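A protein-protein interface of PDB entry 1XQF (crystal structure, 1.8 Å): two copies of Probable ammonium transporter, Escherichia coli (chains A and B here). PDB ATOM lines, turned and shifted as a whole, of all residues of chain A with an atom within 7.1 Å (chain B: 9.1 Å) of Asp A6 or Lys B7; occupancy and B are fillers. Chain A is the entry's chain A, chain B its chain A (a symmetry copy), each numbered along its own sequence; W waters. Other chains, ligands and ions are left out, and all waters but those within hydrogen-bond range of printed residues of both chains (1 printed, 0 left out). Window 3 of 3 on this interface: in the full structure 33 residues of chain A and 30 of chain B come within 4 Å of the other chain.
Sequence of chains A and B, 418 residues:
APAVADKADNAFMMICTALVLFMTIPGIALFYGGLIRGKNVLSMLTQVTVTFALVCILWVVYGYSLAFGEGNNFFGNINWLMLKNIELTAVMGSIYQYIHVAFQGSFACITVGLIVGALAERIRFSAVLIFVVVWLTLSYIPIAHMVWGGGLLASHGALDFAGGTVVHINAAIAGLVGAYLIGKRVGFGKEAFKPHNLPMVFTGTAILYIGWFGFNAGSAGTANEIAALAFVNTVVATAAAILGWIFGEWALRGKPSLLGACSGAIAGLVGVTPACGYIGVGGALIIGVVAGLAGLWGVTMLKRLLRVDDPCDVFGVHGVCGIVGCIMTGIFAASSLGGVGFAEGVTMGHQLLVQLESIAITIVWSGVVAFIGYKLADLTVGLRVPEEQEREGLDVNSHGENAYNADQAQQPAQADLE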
ATOM      1  N   VAL A   4     -15.176 -27.175  31.007  1.00  0.00           N
ATOM      2  CA  VAL A   4     -15.097 -25.832  31.582  1.00  0.00           C
ATOM      3  C   VAL A   4     -16.259 -24.992  31.032  1.00  0.00           C
ATOM      4  O   VAL A   4     -16.667 -25.172  29.883  1.00  0.00           O
ATOM      5  CB  VAL A   4     -13.705 -25.174  31.304  1.00  0.00           C
ATOM      6  CG1 VAL A   4     -13.490 -24.931  29.809  1.00  0.00           C
ATOM      7  CG2 VAL A   4     -13.524 -23.884  32.093  1.00  0.00           C
ATOM      8  N   ALA A   5     -16.810 -24.105  31.861  1.00  0.00           N
ATOM      9  CA  ALA A   5     -17.927 -23.264  31.438  1.00  0.00           C
ATOM     10  C   ALA A   5     -17.469 -22.136  30.510  1.00  0.00           C
ATOM     11  O   ALA A   5     -16.410 -21.542  30.711  1.00  0.00           O
ATOM     12  CB  ALA A   5     -18.674 -22.694  32.653  1.00  0.00           C
ATOM     13  N   ASP A   6     -18.274 -21.874  29.484  1.00  0.00           N
ATOM     14  CA  ASP A   6     -18.064 -20.762  28.556  1.00  0.00           C
ATOM     15  C   ASP A   6     -18.933 -19.578  28.994  1.00  0.00           C
ATOM     16  O   ASP A   6     -20.164 -19.701  29.065  1.00  0.00           O
ATOM     17  CB  ASP A   6     -18.438 -21.214  27.134  1.00  0.00           C
ATOM     18  CG  ASP A   6     -18.202 -20.140  26.078  1.00  0.00           C
ATOM     19  OD1 ASP A   6     -18.827 -19.066  26.144  1.00  0.00           O
ATOM     20  OD2 ASP A   6     -17.413 -20.390  25.144  1.00  0.00           O
ATOM     21  N   LYS A   7     -18.304 -18.433  29.275  1.00  0.00           N
ATOM     22  CA  LYS A   7     -19.045 -17.255  29.820  1.00  0.00           C
ATOM     23  C   LYS A   7     -20.096 -16.646  28.864  1.00  0.00           C
ATOM     24  O   LYS A   7     -21.097 -16.064  29.322  1.00  0.00           O
ATOM     25  CB  LYS A   7     -18.060 -16.173  30.304  1.00  0.00           C
ATOM     26  CG  LYS A   7     -17.362 -16.532  31.622  1.00  0.00           C
ATOM     27  CD  LYS A   7     -16.016 -15.845  31.773  1.00  0.00           C
ATOM     28  CE  LYS A   7     -16.164 -14.398  32.178  1.00  0.00           C
ATOM     29  NZ  LYS A   7     -14.845 -13.708  32.341  1.00  0.00           N
ATOM     30  N   ALA A   8     -19.862 -16.761  27.554  1.00  0.00           N
ATOM     31  CA  ALA A   8     -20.852 -16.319  26.552  1.00  0.00           C
ATOM     32  C   ALA A   8     -22.113 -17.168  26.656  1.00  0.00           C
ATOM     33  O   ALA A   8     -23.219 -16.637  26.603  1.00  0.00           O
ATOM     34  CB  ALA A   8     -20.278 -16.399  25.136  1.00  0.00           C
ATOM     35  N   ASP A   9     -21.938 -18.483  26.801  1.00  0.00           N
ATOM     36  CA  ASP A   9     -23.074 -19.401  27.001  1.00  0.00           C
ATOM     37  C   ASP A   9     -23.781 -19.183  28.365  1.00  0.00           C
ATOM     38  O   ASP A   9     -25.025 -19.230  28.437  1.00  0.00           O
ATOM     39  CB  ASP A   9     -22.618 -20.868  26.822  1.00  0.00           C
ATOM     40  CG  ASP A   9     -22.207 -21.209  25.377  1.00  0.00           C
ATOM     41  OD1 ASP A   9     -22.588 -20.496  24.428  1.00  0.00           O
ATOM     42  OD2 ASP A   9     -21.504 -22.224  25.184  1.00  0.00           O
ATOM     43  N   ASN A  10     -23.005 -18.938  29.426  1.00  0.00           N
ATOM     44  CA  ASN A  10     -23.558 -18.575  30.759  1.00  0.00           C
ATOM     45  C   ASN A  10     -24.476 -17.331  30.679  1.00  0.00           C
ATOM     46  O   ASN A  10     -25.590 -17.314  31.221  1.00  0.00           O
ATOM     47  CB  ASN A  10     -22.441 -18.276  31.782  1.00  0.00           C
ATOM     48  CG  ASN A  10     -21.695 -19.530  32.285  1.00  0.00           C
ATOM     49  OD1 ASN A  10     -22.188 -20.656  32.228  1.00  0.00           O
ATOM     50  ND2 ASN A  10     -20.494 -19.309  32.806  1.00  0.00           N
ATOM     51  N   ALA A  11     -23.986 -16.294  30.007  1.00  0.00           N
ATOM     52  CA  ALA A  11     -24.743 -15.045  29.791  1.00  0.00           C
ATOM     53  C   ALA A  11     -26.055 -15.257  29.016  1.00  0.00           C
ATOM     54  O   ALA A  11     -27.123 -14.833  29.481  1.00  0.00           O
ATOM     55  CB  ALA A  11     -23.859 -14.020  29.079  1.00  0.00           C
ATOM     56  N   PHE A  12     -25.965 -15.918  27.853  1.00  0.00           N
ATOM     57  CA  PHE A  12     -27.118 -16.230  27.001  1.00  0.00           C
ATOM     58  C   PHE A  12     -28.205 -16.996  27.765  1.00  0.00           C
ATOM     59  O   PHE A  12     -29.397 -16.654  27.685  1.00  0.00           O
ATOM     60  CB  PHE A  12     -26.661 -17.050  25.769  1.00  0.00           C
ATOM     61  CG  PHE A  12     -27.761 -17.333  24.754  1.00  0.00           C
ATOM     62  CD1 PHE A  12     -28.425 -16.289  24.110  1.00  0.00           C
ATOM     63  CD2 PHE A  12     -28.089 -18.655  24.412  1.00  0.00           C
ATOM     64  CE1 PHE A  12     -29.431 -16.555  23.162  1.00  0.00           C
ATOM     65  CE2 PHE A  12     -29.077 -18.935  23.464  1.00  0.00           C
ATOM     66  CZ  PHE A  12     -29.751 -17.892  22.842  1.00  0.00           C
ATOM     67  N   VAL A  91     -20.118 -28.142  35.877  1.00  0.00           N
ATOM     68  CA  VAL A  91     -20.533 -27.784  34.515  1.00  0.00           C
ATOM     69  C   VAL A  91     -21.486 -28.838  33.946  1.00  0.00           C
ATOM     70  O   VAL A  91     -21.260 -30.047  34.117  1.00  0.00           O
ATOM     71  CB  VAL A  91     -19.284 -27.643  33.589  1.00  0.00           C
ATOM     72  CG1 VAL A  91     -19.673 -27.350  32.136  1.00  0.00           C
ATOM     73  CG2 VAL A  91     -18.341 -26.577  34.126  1.00  0.00           C
ATOM     74  N   GLY A  93     -22.988 -29.549  30.148  1.00  0.00           N
ATOM     75  CA  GLY A  93     -22.846 -29.095  28.753  1.00  0.00           C
ATOM     76  C   GLY A  93     -21.723 -28.077  28.650  1.00  0.00           C
ATOM     77  O   GLY A  93     -20.554 -28.430  28.854  1.00  0.00           O
ATOM     78  N   SER A  94     -22.073 -26.817  28.354  1.00  0.00           N
ATOM     79  CA  SER A  94     -21.094 -25.717  28.337  1.00  0.00           C
ATOM     80  C   SER A  94     -21.420 -24.564  29.305  1.00  0.00           C
ATOM     81  O   SER A  94     -20.892 -23.448  29.167  1.00  0.00           O
ATOM     82  CB  SER A  94     -20.863 -25.197  26.905  1.00  0.00           C
ATOM     83  OG  SER A  94     -22.047 -24.655  26.341  1.00  0.00           O
ATOM     84  N   ILE A  95     -22.284 -24.831  30.287  1.00  0.00           N
ATOM     85  CA  ILE A  95     -22.680 -23.809  31.275  1.00  0.00           C
ATOM     86  C   ILE A  95     -22.594 -24.360  32.710  1.00  0.00           C
ATOM     87  O   ILE A  95     -22.521 -25.569  32.896  1.00  0.00           O
ATOM     88  CB  ILE A  95     -24.123 -23.254  31.015  1.00  0.00           C
ATOM     89  CG1 ILE A  95     -25.182 -24.375  31.123  1.00  0.00           C
ATOM     90  CG2 ILE A  95     -24.189 -22.503  29.670  1.00  0.00           C
ATOM     91  CD1 ILE A  95     -26.664 -23.891  31.087  1.00  0.00           C
ATOM     92  N   TYR A  96     -22.594 -23.474  33.711  1.00  0.00           N
ATOM     93  CA  TYR A  96     -22.669 -23.904  35.125  1.00  0.00           C
ATOM     94  C   TYR A  96     -24.003 -24.614  35.391  1.00  0.00           C
ATOM     95  O   TYR A  96     -25.070 -24.176  34.921  1.00  0.00           O
ATOM     96  CB  TYR A  96     -22.432 -22.729  36.102  1.00  0.00           C
ATOM     97  CG  TYR A  96     -20.985 -22.247  36.107  1.00  0.00           C
ATOM     98  CD1 TYR A  96     -19.949 -23.095  36.518  1.00  0.00           C
ATOM     99  CD2 TYR A  96     -20.646 -20.947  35.687  1.00  0.00           C
ATOM    100  CE1 TYR A  96     -18.621 -22.675  36.515  1.00  0.00           C
ATOM    101  CE2 TYR A  96     -19.295 -20.514  35.684  1.00  0.00           C
ATOM    102  CZ  TYR A  96     -18.298 -21.393  36.097  1.00  0.00           C
ATOM    103  OH  TYR A  96     -16.972 -21.004  36.106  1.00  0.00           O
ATOM    104  N   ILE A  99     -27.214 -22.864  36.443  1.00  0.00           N
ATOM    105  CA  ILE A  99     -27.980 -22.208  35.362  1.00  0.00           C
ATOM    106  C   ILE A  99     -28.942 -23.193  34.678  1.00  0.00           C
ATOM    107  O   ILE A  99     -30.079 -22.837  34.373  1.00  0.00           O
ATOM    108  CB  ILE A  99     -27.067 -21.490  34.306  1.00  0.00           C
ATOM    109  CG1 ILE A  99     -26.180 -20.438  34.971  1.00  0.00           C
ATOM    110  CG2 ILE A  99     -27.903 -20.790  33.216  1.00  0.00           C
ATOM    111  CD1 ILE A  99     -25.065 -19.887  34.054  1.00  0.00           C
ATOM    112  N   THR A 222     -26.544 -23.078  24.211  1.00  0.00           N
ATOM    113  CA  THR A 222     -25.334 -22.364  23.784  1.00  0.00           C
ATOM    114  C   THR A 222     -25.695 -21.302  22.728  1.00  0.00           C
ATOM    115  O   THR A 222     -26.640 -21.486  21.965  1.00  0.00           O
ATOM    116  CB  THR A 222     -24.229 -23.352  23.237  1.00  0.00           C
ATOM    117  OG1 THR A 222     -23.156 -22.624  22.610  1.00  0.00           O
ATOM    118  CG2 THR A 222     -24.806 -24.361  22.230  1.00  0.00           C
ATOM    119  N   ALA A 223     -24.944 -20.201  22.681  1.00  0.00           N
ATOM    120  CA  ALA A 223     -25.159 -19.165  21.650  1.00  0.00           C
ATOM    121  C   ALA A 223     -24.474 -19.498  20.301  1.00  0.00           C
ATOM    122  O   ALA A 223     -23.542 -18.800  19.864  1.00  0.00           O
ATOM    123  CB  ALA A 223     -24.728 -17.761  22.180  1.00  0.00           C
ATOM    124  N   ASN A 224     -24.949 -20.559  19.644  1.00  0.00           N
ATOM    125  CA  ASN A 224     -24.355 -21.061  18.397  1.00  0.00           C
ATOM    126  C   ASN A 224     -25.290 -20.963  17.168  1.00  0.00           C
ATOM    127  O   ASN A 224     -26.284 -20.229  17.195  1.00  0.00           O
ATOM    128  CB  ASN A 224     -23.838 -22.499  18.602  1.00  0.00           C
ATOM    129  CG  ASN A 224     -24.961 -23.542  18.715  1.00  0.00           C
ATOM    130  OD1 ASN A 224     -26.137 -23.212  18.852  1.00  0.00           O
ATOM    131  ND2 ASN A 224     -24.582 -24.819  18.654  1.00  0.00           N
ATOM    132  N   VAL B   4     -14.601 -16.334  11.735  1.00  0.00           N
ATOM    133  CA  VAL B   4     -15.260 -17.256  12.660  1.00  0.00           C
ATOM    134  C   VAL B   4     -16.187 -16.450  13.582  1.00  0.00           C
ATOM    135  O   VAL B   4     -15.878 -15.308  13.929  1.00  0.00           O
ATOM    136  CB  VAL B   4     -14.215 -18.101  13.461  1.00  0.00           C
ATOM    137  CG1 VAL B   4     -13.369 -17.220  14.383  1.00  0.00           C
ATOM    138  CG2 VAL B   4     -14.882 -19.223  14.248  1.00  0.00           C
ATOM    139  N   ALA B   5     -17.330 -17.028  13.947  1.00  0.00           N
ATOM    140  CA  ALA B   5     -18.286 -16.343  14.813  1.00  0.00           C
ATOM    141  C   ALA B   5     -17.815 -16.319  16.270  1.00  0.00           C
ATOM    142  O   ALA B   5     -17.258 -17.296  16.770  1.00  0.00           O
ATOM    143  CB  ALA B   5     -19.678 -16.980  14.706  1.00  0.00           C
ATOM    144  N   ASP B   6     -18.031 -15.181  16.925  1.00  0.00           N
ATOM    145  CA  ASP B   6     -17.755 -15.006  18.350  1.00  0.00           C
ATOM    146  C   ASP B   6     -19.053 -15.212  19.137  1.00  0.00           C
ATOM    147  O   ASP B   6     -20.037 -14.492  18.916  1.00  0.00           O
ATOM    148  CB  ASP B   6     -17.195 -13.593  18.586  1.00  0.00           C
ATOM    149  CG  ASP B   6     -16.821 -13.326  20.040  1.00  0.00           C
ATOM    150  OD1 ASP B   6     -17.702 -13.367  20.918  1.00  0.00           O
ATOM    151  OD2 ASP B   6     -15.638 -13.026  20.302  1.00  0.00           O
ATOM    152  N   LYS B   7     -19.059 -16.178  20.060  1.00  0.00           N
ATOM    153  CA  LYS B   7     -20.306 -16.536  20.801  1.00  0.00           C
ATOM    154  C   LYS B   7     -20.866 -15.421  21.714  1.00  0.00           C
ATOM    155  O   LYS B   7     -22.087 -15.360  21.951  1.00  0.00           O
ATOM    156  CB  LYS B   7     -20.108 -17.841  21.597  1.00  0.00           C
ATOM    157  CG  LYS B   7     -20.093 -19.095  20.715  1.00  0.00           C
ATOM    158  CD  LYS B   7     -19.311 -20.237  21.339  1.00  0.00           C
ATOM    159  CE  LYS B   7     -20.100 -20.936  22.422  1.00  0.00           C
ATOM    160  NZ  LYS B   7     -19.345 -22.072  23.042  1.00  0.00           N
ATOM    161  N   ALA B   8     -19.983 -14.564  22.235  1.00  0.00           N
ATOM    162  CA  ALA B   8     -20.416 -13.395  23.025  1.00  0.00           C
ATOM    163  C   ALA B   8     -21.207 -12.435  22.145  1.00  0.00           C
ATOM    164  O   ALA B   8     -22.240 -11.921  22.567  1.00  0.00           O
ATOM    165  CB  ALA B   8     -19.219 -12.675  23.648  1.00  0.00           C
ATOM    166  N   ASP B   9     -20.716 -12.200  20.926  1.00  0.00           N
ATOM    167  CA  ASP B   9     -21.431 -11.360  19.949  1.00  0.00           C
ATOM    168  C   ASP B   9     -22.754 -12.010  19.464  1.00  0.00           C
ATOM    169  O   ASP B   9     -23.774 -11.309  19.308  1.00  0.00           O
ATOM    170  CB  ASP B   9     -20.503 -11.003  18.765  1.00  0.00           C
ATOM    171  CG  ASP B   9     -19.338 -10.075  19.160  1.00  0.00           C
ATOM    172  OD1 ASP B   9     -19.397  -9.398  20.205  1.00  0.00           O
ATOM    173  OD2 ASP B   9     -18.350 -10.007  18.398  1.00  0.00           O
ATOM    174  N   ASN B  10     -22.743 -13.328  19.239  1.00  0.00           N
ATOM    175  CA  ASN B  10     -23.974 -14.097  18.906  1.00  0.00           C
ATOM    176  C   ASN B  10     -25.071 -13.916  19.984  1.00  0.00           C
ATOM    177  O   ASN B  10     -26.243 -13.656  19.675  1.00  0.00           O
ATOM    178  CB  ASN B  10     -23.688 -15.608  18.769  1.00  0.00           C
ATOM    179  CG  ASN B  10     -22.938 -15.993  17.477  1.00  0.00           C
ATOM    180  OD1 ASN B  10     -22.942 -15.277  16.476  1.00  0.00           O
ATOM    181  ND2 ASN B  10     -22.307 -17.160  17.508  1.00  0.00           N
ATOM    182  N   ALA B  11     -24.675 -14.068  21.243  1.00  0.00           N
ATOM    183  CA  ALA B  11     -25.577 -13.884  22.397  1.00  0.00           C
ATOM    184  C   ALA B  11     -26.172 -12.469  22.484  1.00  0.00           C
ATOM    185  O   ALA B  11     -27.398 -12.319  22.574  1.00  0.00           O
ATOM    186  CB  ALA B  11     -24.839 -14.237  23.691  1.00  0.00           C
ATOM    187  N   PHE B  12     -25.302 -11.449  22.445  1.00  0.00           N
ATOM    188  CA  PHE B  12     -25.698 -10.036  22.489  1.00  0.00           C
ATOM    189  C   PHE B  12     -26.708  -9.691  21.388  1.00  0.00           C
ATOM    190  O   PHE B  12     -27.735  -9.040  21.649  1.00  0.00           O
ATOM    191  CB  PHE B  12     -24.449  -9.131  22.364  1.00  0.00           C
ATOM    192  CG  PHE B  12     -24.731  -7.640  22.513  1.00  0.00           C
ATOM    193  CD1 PHE B  12     -25.277  -7.130  23.691  1.00  0.00           C
ATOM    194  CD2 PHE B  12     -24.396  -6.747  21.482  1.00  0.00           C
ATOM    195  CE1 PHE B  12     -25.522  -5.751  23.831  1.00  0.00           C
ATOM    196  CE2 PHE B  12     -24.623  -5.375  21.610  1.00  0.00           C
ATOM    197  CZ  PHE B  12     -25.187  -4.874  22.776  1.00  0.00           C
ATOM    198  N   MET B  13     -26.408 -10.121  20.166  1.00  0.00           N
ATOM    199  CA  MET B  13     -27.215  -9.773  18.982  1.00  0.00           C
ATOM    200  C   MET B  13     -28.574 -10.501  18.893  1.00  0.00           C
ATOM    201  O   MET B  13     -29.543  -9.918  18.407  1.00  0.00           O
ATOM    202  CB  MET B  13     -26.388  -9.931  17.690  1.00  0.00           C
ATOM    203  CG  MET B  13     -25.237  -8.905  17.557  1.00  0.00           C
ATOM    204  SD  MET B  13     -25.753  -7.154  17.583  1.00  0.00           S
ATOM    205  CE  MET B  13     -26.956  -7.086  16.252  1.00  0.00           C
ATOM    206  N   MET B  14     -28.652 -11.755  19.357  1.00  0.00           N
ATOM    207  CA  MET B  14     -29.956 -12.430  19.514  1.00  0.00           C
ATOM    208  C   MET B  14     -30.869 -11.727  20.556  1.00  0.00           C
ATOM    209  O   MET B  14     -32.063 -11.520  20.303  1.00  0.00           O
ATOM    210  CB  MET B  14     -29.791 -13.934  19.837  1.00  0.00           C
ATOM    211  CG  MET B  14     -29.415 -14.805  18.612  1.00  0.00           C
ATOM    212  SD  MET B  14     -29.392 -16.600  18.861  1.00  0.00           S
ATOM    213  CE  MET B  14     -27.835 -16.811  19.768  1.00  0.00           C
ATOM    214  N   ILE B  15     -30.310 -11.348  21.702  1.00  0.00           N
ATOM    215  CA  ILE B  15     -31.101 -10.629  22.741  1.00  0.00           C
ATOM    216  C   ILE B  15     -31.534  -9.225  22.249  1.00  0.00           C
ATOM    217  O   ILE B  15     -32.676  -8.805  22.489  1.00  0.00           O
ATOM    218  CB  ILE B  15     -30.374 -10.553  24.136  1.00  0.00           C
ATOM    219  CG1 ILE B  15     -29.989 -11.948  24.669  1.00  0.00           C
ATOM    220  CG2 ILE B  15     -31.241  -9.829  25.195  1.00  0.00           C
ATOM    221  CD1 ILE B  15     -31.155 -12.944  24.842  1.00  0.00           C
ATOM    222  N   SER B  94     -18.918 -10.426  12.833  1.00  0.00           N
ATOM    223  CA  SER B  94     -18.479 -11.368  13.877  1.00  0.00           C
ATOM    224  C   SER B  94     -19.598 -12.273  14.425  1.00  0.00           C
ATOM    225  O   SER B  94     -19.465 -12.863  15.511  1.00  0.00           O
ATOM    226  CB  SER B  94     -17.743 -10.636  15.015  1.00  0.00           C
ATOM    227  OG  SER B  94     -18.584  -9.706  15.678  1.00  0.00           O
ATOM    228  N   ILE B  95     -20.698 -12.386  13.679  1.00  0.00           N
ATOM    229  CA  ILE B  95     -21.842 -13.219  14.099  1.00  0.00           C
ATOM    230  C   ILE B  95     -22.317 -14.131  12.953  1.00  0.00           C
ATOM    231  O   ILE B  95     -21.962 -13.900  11.803  1.00  0.00           O
ATOM    232  CB  ILE B  95     -23.048 -12.362  14.616  1.00  0.00           C
ATOM    233  CG1 ILE B  95     -23.591 -11.433  13.507  1.00  0.00           C
ATOM    234  CG2 ILE B  95     -22.667 -11.595  15.899  1.00  0.00           C
ATOM    235  CD1 ILE B  95     -24.919 -10.691  13.854  1.00  0.00           C
ATOM    236  N   TYR B  96     -23.104 -15.163  13.272  1.00  0.00           N
ATOM    237  CA  TYR B  96     -23.737 -16.004  12.231  1.00  0.00           C
ATOM    238  C   TYR B  96     -24.712 -15.166  11.394  1.00  0.00           C
ATOM    239  O   TYR B  96     -25.473 -14.339  11.931  1.00  0.00           O
ATOM    240  CB  TYR B  96     -24.415 -17.257  12.833  1.00  0.00           C
ATOM    241  CG  TYR B  96     -23.412 -18.282  13.351  1.00  0.00           C
ATOM    242  CD1 TYR B  96     -22.514 -18.911  12.478  1.00  0.00           C
ATOM    243  CD2 TYR B  96     -23.348 -18.617  14.716  1.00  0.00           C
ATOM    244  CE1 TYR B  96     -21.582 -19.837  12.937  1.00  0.00           C
ATOM    245  CE2 TYR B  96     -22.402 -19.564  15.188  1.00  0.00           C
ATOM    246  CZ  TYR B  96     -21.526 -20.159  14.285  1.00  0.00           C
ATOM    247  OH  TYR B  96     -20.592 -21.084  14.710  1.00  0.00           O
ATOM    248  N   ILE B  99     -28.380 -14.624  12.245  1.00  0.00           N
ATOM    249  CA  ILE B  99     -28.664 -13.603  13.276  1.00  0.00           C
ATOM    250  C   ILE B  99     -28.775 -12.198  12.660  1.00  0.00           C
ATOM    251  O   ILE B  99     -29.648 -11.422  13.042  1.00  0.00           O
ATOM    252  CB  ILE B  99     -27.632 -13.616  14.459  1.00  0.00           C
ATOM    253  CG1 ILE B  99     -27.593 -14.985  15.138  1.00  0.00           C
ATOM    254  CG2 ILE B  99     -27.981 -12.563  15.528  1.00  0.00           C
ATOM    255  CD1 ILE B  99     -26.416 -15.164  16.123  1.00  0.00           C
ATOM    256  N   ALA B 223     -20.505  -6.826  21.121  1.00  0.00           N
ATOM    257  CA  ALA B 223     -20.494  -6.296  22.501  1.00  0.00           C
ATOM    258  C   ALA B 223     -19.159  -5.605  22.876  1.00  0.00           C
ATOM    259  O   ALA B 223     -18.417  -6.076  23.756  1.00  0.00           O
ATOM    260  CB  ALA B 223     -20.867  -7.415  23.524  1.00  0.00           C
HETATM  261  O   HOH W   1     -21.223 -24.048  21.224  1.00  0.00           O
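Among the printed residues, merely in contact across the chains: Ala A8 with Lys B7, Ala A8 with Ala B8, Phe A12 with Ala B11, Phe A12 with Met B14, Thr A222 with Lys B7, Ala A223 with Lys B7, Ala A223 with Ala B11 and Asn A224 with Tyr B96.
Water W1 bridges the side-chain hydroxyl (OG1) of Thr A222 (2.8 Å) and the side-chain amino group (NZ) of Lys B7 (3.3 Å).
The backbone NH (N) of Ala A223 lies within hydrogen-bond range of the side-chain carboxylate (OD1) of Asp A9 (2.9 Å). N of Asp A6 is in hydrogen-bond range of O of Ser A94 (3.1 Å). OD1 of Asp A9 lies within hydrogen-bond range of OG1 of Thr A222 (2.9 Å). The side-chain carboxylate (OD1) of Asp A6 lies within hydrogen-bond range of the backbone NH (N) of Ala A8 (2.9 Å). OD1 of Asp B6 is in hydrogen-bond range of N of Ala B8 (2.9 Å). The side-chain carboxylate (OD1) of Asp A6 is in hydrogen-bond range of the backbone NH (N) of Asp A9.
Of the 17 printed residues of chain B, 6 touch a printed residue of chain A. Along chain B the printed residues that touch a printed residue of chain A span positions 7 to 96. Of the 18 printed residues of chain A, 7 touch a printed residue of chain B. Printed residues of chain A that touch a printed residue of chain B: Asp A6, Ala A8, Asp A9, Phe A12, Thr A222, Ala A223 and Asn A224. Hydrophobic or aromatic side chains of chain A within 4 Å of the printed part of chain B: Ala A8, Phe A12 and Ala A223. Among the printed residues, 11 pairs touch across the chains. Among the printed residues, Asp or Glu carboxylates within 4 Å of a Lys or Arg side-chain nitrogen of the other chain: Asp A6 with Lys B7 (3.3 Å) and Asp A9 with Lys B7 (3.0 Å).
Of chain B, only Lys B7 comes within 4 Å of Asp A6. Printed residues of chain B within 4 Å of Ala A8: Lys B7 and Ala B8. Asp A9 touches just one residue of chain B: Lys B7. Ala A223 touches just these residues of chain B: Lys B7, Asn B10 and Ala B11. Of the printed residues of chain B, Asn A224 touches Tyr B96. Ala B5 touches none of the printed residues of chain A. Lys B7 touches just these residues of chain A: Asp A6 (3.3 Å), Ala A8 (3.6 Å), Asp A9 (3.0 Å), Thr A222 (3.5 Å) and Ala A223 (3.6 Å). Printed residues of chain A within 4 Å of Ala B8: Ala A8. Printed residues of chain A within 4 Å of Met B14: Phe A12. Ser B94 touches none of the printed residues of chain A. The nearest residue of chain A that does not touch Lys B7 is Ser A94 (5.0 Å).
The side-chain amino group (NZ) of Lys B7 lies within salt-bridge range of the side-chain carboxylate (OD2) of Asp A9, at 3.0 Å. NZ of Lys B7 is in salt-bridge range of OD2 of Asp A6 (3.3 Å). The side-chain amide nitrogen (ND2) of Asn B10 sits at hydrogen-bond distance from the backbone carbonyl oxygen (O) of Ala A223, 3.1 Å away.
Ala B8 touches its own counterpart, Ala A8. Phe A12 touches Ala B11, but with the chains exchanged Ala A11 does not touch Phe B12 (7.3 Å). Ala A223 touches Asn B10, but with the chains exchanged Asn A10 does not touch Ala B223 (12.7 Å). Ala A223 touches Ala B11, but with the chains exchanged Ala A11 does not touch Ala B223 (9.1 Å). Positions printed for both chains: 4, 5, 6, 7, 8, 9, 10, 11, 12, 94, 95, 96, 99 and 223. Of the 11 pairs that touch across the chains among the printed residues, 1 has its exchanged pair printed and touching as well.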
